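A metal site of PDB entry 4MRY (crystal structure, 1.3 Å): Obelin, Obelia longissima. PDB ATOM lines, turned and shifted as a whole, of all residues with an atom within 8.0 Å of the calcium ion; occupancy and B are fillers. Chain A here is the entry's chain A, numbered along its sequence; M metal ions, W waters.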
ATOM      1  N   THR A 129      27.258  -5.597 -31.632  1.00  0.00           N
ATOM      2  CA  THR A 129      26.769  -4.620 -30.659  1.00  0.00           C
ATOM      3  C   THR A 129      26.526  -5.360 -29.377  1.00  0.00           C
ATOM      4  O   THR A 129      26.266  -6.522 -29.424  1.00  0.00           O
ATOM      5  CB  THR A 129      25.431  -4.017 -31.102  1.00  0.00           C
ATOM      6  OG1 THR A 129      24.492  -5.071 -31.307  1.00  0.00           O
ATOM      7  CG2 THR A 129      25.608  -3.228 -32.397  1.00  0.00           C
ATOM      8  N   ILE A 130      26.593  -4.709 -28.230  1.00  0.00           N
ATOM      9  CA  ILE A 130      26.196  -5.382 -27.001  1.00  0.00           C
ATOM     10  C   ILE A 130      24.830  -4.853 -26.542  1.00  0.00           C
ATOM     11  O   ILE A 130      24.662  -3.648 -26.353  1.00  0.00           O
ATOM     12  CB  ILE A 130      27.218  -5.187 -25.854  1.00  0.00           C
ATOM     13  CG1 ILE A 130      28.557  -5.822 -26.210  1.00  0.00           C
ATOM     14  CG2 ILE A 130      26.701  -5.765 -24.545  1.00  0.00           C
ATOM     15  CD1 ILE A 130      29.622  -5.558 -25.168  1.00  0.00           C
ATOM     16  N   PHE A 155      24.760  -0.028 -17.810  1.00  0.00           N
ATOM     17  CA  PHE A 155      24.517  -0.026 -19.247  1.00  0.00           C
ATOM     18  C   PHE A 155      24.213   1.384 -19.737  1.00  0.00           C
ATOM     19  O   PHE A 155      24.757   1.843 -20.736  1.00  0.00           O
ATOM     20  CB  PHE A 155      23.365  -0.968 -19.590  1.00  0.00           C
ATOM     21  CG  PHE A 155      23.147  -1.160 -21.058  1.00  0.00           C
ATOM     22  CD1 PHE A 155      23.852  -2.127 -21.762  1.00  0.00           C
ATOM     23  CD2 PHE A 155      22.217  -0.384 -21.753  1.00  0.00           C
ATOM     24  CE1 PHE A 155      23.648  -2.321 -23.123  1.00  0.00           C
ATOM     25  CE2 PHE A 155      22.008  -0.569 -23.113  1.00  0.00           C
ATOM     26  CZ  PHE A 155      22.729  -1.540 -23.802  1.00  0.00           C
ATOM     27  N   CYS A 158      27.157   3.561 -20.052  1.00  0.00           N
ATOM     28  CA  CYS A 158      27.948   3.223 -21.246  1.00  0.00           C
ATOM     29  C   CYS A 158      27.323   3.714 -22.518  1.00  0.00           C
ATOM     30  O   CYS A 158      28.027   4.129 -23.447  1.00  0.00           O
ATOM     31  CB  CYS A 158      28.114   1.708 -21.386  1.00  0.00           C
ATOM     32  SG  CYS A 158      29.235   0.940 -20.232  1.00  0.00           S
ATOM     33  N   ASP A 159      26.004   3.633 -22.591  1.00  0.00           N
ATOM     34  CA  ASP A 159      25.274   3.879 -23.843  1.00  0.00           C
ATOM     35  C   ASP A 159      25.106   5.388 -24.116  1.00  0.00           C
ATOM     36  O   ASP A 159      24.020   5.952 -23.964  1.00  0.00           O
ATOM     37  CB  ASP A 159      23.923   3.139 -23.773  1.00  0.00           C
ATOM     38  CG  ASP A 159      23.167   3.169 -25.075  1.00  0.00           C
ATOM     39  OD1 ASP A 159      23.750   3.623 -26.050  1.00  0.00           O
ATOM     40  OD2 ASP A 159      22.008   2.753 -25.141  1.00  0.00           O
ATOM     41  N   LEU A 160      26.196   6.026 -24.538  1.00  0.00           N
ATOM     42  CA  LEU A 160      26.242   7.487 -24.654  1.00  0.00           C
ATOM     43  C   LEU A 160      25.224   8.080 -25.620  1.00  0.00           C
ATOM     44  O   LEU A 160      24.705   9.170 -25.370  1.00  0.00           O
ATOM     45  CB  LEU A 160      27.644   7.955 -25.066  1.00  0.00           C
ATOM     46  CG  LEU A 160      28.810   7.616 -24.132  1.00  0.00           C
ATOM     47  CD1 LEU A 160      30.072   8.342 -24.571  1.00  0.00           C
ATOM     48  CD2 LEU A 160      28.482   7.908 -22.665  1.00  0.00           C
ATOM     49  N   ASP A 161      24.917   7.395 -26.699  1.00  0.00           N
ATOM     50  CA  ASP A 161      23.940   7.960 -27.636  1.00  0.00           C
ATOM     51  C   ASP A 161      22.543   7.366 -27.427  1.00  0.00           C
ATOM     52  O   ASP A 161      21.633   7.602 -28.235  1.00  0.00           O
ATOM     53  CB  ASP A 161      24.420   7.832 -29.085  1.00  0.00           C
ATOM     54  CG  ASP A 161      24.533   6.402 -29.533  1.00  0.00           C
ATOM     55  OD1 ASP A 161      24.282   5.534 -28.691  1.00  0.00           O
ATOM     56  OD2 ASP A 161      24.879   6.140 -30.697  1.00  0.00           O
ATOM     57  N   ASN A 162      22.363   6.632 -26.326  1.00  0.00           N
ATOM     58  CA  ASN A 162      21.088   5.996 -25.993  1.00  0.00           C
ATOM     59  C   ASN A 162      20.497   5.260 -27.187  1.00  0.00           C
ATOM     60  O   ASN A 162      19.314   5.386 -27.502  1.00  0.00           O
ATOM     61  CB  ASN A 162      20.069   6.987 -25.427  1.00  0.00           C
ATOM     62  CG  ASN A 162      18.846   6.303 -24.861  1.00  0.00           C
ATOM     63  OD1 ASN A 162      18.939   5.153 -24.394  1.00  0.00           O
ATOM     64  ND2 ASN A 162      17.705   6.965 -24.902  1.00  0.00           N
ATOM     65  N   SER A 163      21.325   4.465 -27.852  1.00  0.00           N
ATOM     66  CA  SER A 163      20.865   3.684 -28.992  1.00  0.00           C
ATOM     67  C   SER A 163      20.243   2.384 -28.533  1.00  0.00           C
ATOM     68  O   SER A 163      19.592   1.693 -29.327  1.00  0.00           O
ATOM     69  CB  SER A 163      22.026   3.358 -29.907  1.00  0.00           C
ATOM     70  OG  SER A 163      22.847   2.385 -29.280  1.00  0.00           O
ATOM     71  N   GLY A 164      20.445   2.015 -27.275  1.00  0.00           N
ATOM     72  CA  GLY A 164      19.953   0.748 -26.784  1.00  0.00           C
ATOM     73  C   GLY A 164      20.915  -0.414 -26.971  1.00  0.00           C
ATOM     74  O   GLY A 164      20.573  -1.567 -26.708  1.00  0.00           O
ATOM     75  N   ASP A 165      22.130  -0.113 -27.424  1.00  0.00           N
ATOM     76  CA  ASP A 165      23.154  -1.141 -27.581  1.00  0.00           C
ATOM     77  C   ASP A 165      24.506  -0.492 -27.431  1.00  0.00           C
ATOM     78  O   ASP A 165      24.588   0.689 -27.550  1.00  0.00           O
ATOM     79  CB  ASP A 165      23.019  -1.874 -28.939  1.00  0.00           C
ATOM     80  CG  ASP A 165      23.016  -0.940 -30.146  1.00  0.00           C
ATOM     81  OD1 ASP A 165      23.288   0.266 -30.030  1.00  0.00           O
ATOM     82  OD2 ASP A 165      22.732  -1.438 -31.256  1.00  0.00           O
ATOM     83  N   LEU A 166      25.574  -1.226 -27.130  1.00  0.00           N
ATOM     84  CA  LEU A 166      26.893  -0.602 -26.999  1.00  0.00           C
ATOM     85  C   LEU A 166      27.792  -0.981 -28.162  1.00  0.00           C
ATOM     86  O   LEU A 166      27.777  -2.152 -28.594  1.00  0.00           O
ATOM     87  CB  LEU A 166      27.582  -1.034 -25.690  1.00  0.00           C
ATOM     88  CG  LEU A 166      26.721  -1.070 -24.443  1.00  0.00           C
ATOM     89  CD1 LEU A 166      27.512  -1.601 -23.264  1.00  0.00           C
ATOM     90  CD2 LEU A 166      26.144   0.319 -24.126  1.00  0.00           C
ATOM     91  N   ASP A 167      28.589  -0.040 -28.659  1.00  0.00           N
ATOM     92  CA  ASP A 167      29.680  -0.409 -29.546  1.00  0.00           C
ATOM     93  C   ASP A 167      30.998  -0.509 -28.758  1.00  0.00           C
ATOM     94  O   ASP A 167      31.028  -0.217 -27.547  1.00  0.00           O
ATOM     95  CB  ASP A 167      29.770   0.481 -30.802  1.00  0.00           C
ATOM     96  CG  ASP A 167      30.097   1.928 -30.496  1.00  0.00           C
ATOM     97  OD1 ASP A 167      30.481   2.259 -29.353  1.00  0.00           O
ATOM     98  OD2 ASP A 167      29.992   2.765 -31.427  1.00  0.00           O
ATOM     99  N   GLU A 170      32.096   2.745 -27.047  1.00  0.00           N
ATOM    100  CA  GLU A 170      31.373   3.079 -25.829  1.00  0.00           C
ATOM    101  C   GLU A 170      31.860   2.281 -24.636  1.00  0.00           C
ATOM    102  O   GLU A 170      32.097   2.827 -23.568  1.00  0.00           O
ATOM    103  CB  GLU A 170      29.882   2.886 -26.022  1.00  0.00           C
ATOM    104  CG  GLU A 170      29.313   3.983 -26.842  1.00  0.00           C
ATOM    105  CD  GLU A 170      27.887   3.780 -27.096  1.00  0.00           C
ATOM    106  OE1 GLU A 170      27.472   2.607 -27.004  1.00  0.00           O
ATOM    107  OE2 GLU A 170      27.185   4.793 -27.384  1.00  0.00           O
ATOM    108  N   MET A 171      32.031   0.979 -24.813  1.00  0.00           N
ATOM    109  CA  MET A 171      32.524   0.136 -23.717  1.00  0.00           C
ATOM    110  C   MET A 171      33.929   0.526 -23.290  1.00  0.00           C
ATOM    111  O   MET A 171      34.234   0.656 -22.107  1.00  0.00           O
ATOM    112  CB  MET A 171      32.475  -1.348 -24.088  1.00  0.00           C
ATOM    113  CG  MET A 171      32.735  -2.245 -22.897  1.00  0.00           C
ATOM    114  SD  MET A 171      32.733  -3.992 -23.297  1.00  0.00           S
ATOM    115  CE  MET A 171      34.228  -4.113 -24.257  1.00  0.00           C
HETATM  116 CA    CA M   1      25.143   3.178 -28.064  1.00  0.00          CA
HETATM  117  O   HOH W   1      25.996   2.638 -30.071  1.00  0.00           O
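The side-chain carboxylate (OD1) of Asp 159 sits close to the backbone NH (N) of Asn 162 (3.3 Å).
OD2 of Asp 159 is in hydrogen-bond range of N of Gly 164 (2.7 Å).
The backbone NH (N) of Leu 160 sits close to the side-chain carboxylate (OE2) of Glu 170.
The backbone NH (N) of Glu 170 lies within hydrogen-bond range of the side-chain carboxylate (OD1) of Asp 167 (2.9 Å).
Of the 15 residues printed, 5 come within 4 Å of the calcium ion.
The calcium ion is bound by water W1, OD1 of Asp 159, OD1 of Asp 161, O of Asp 165, OE1 of Glu 170, OE2 of Glu 170 and OG of Ser 163.
The calcium ion has seven donor atoms within binding distance.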
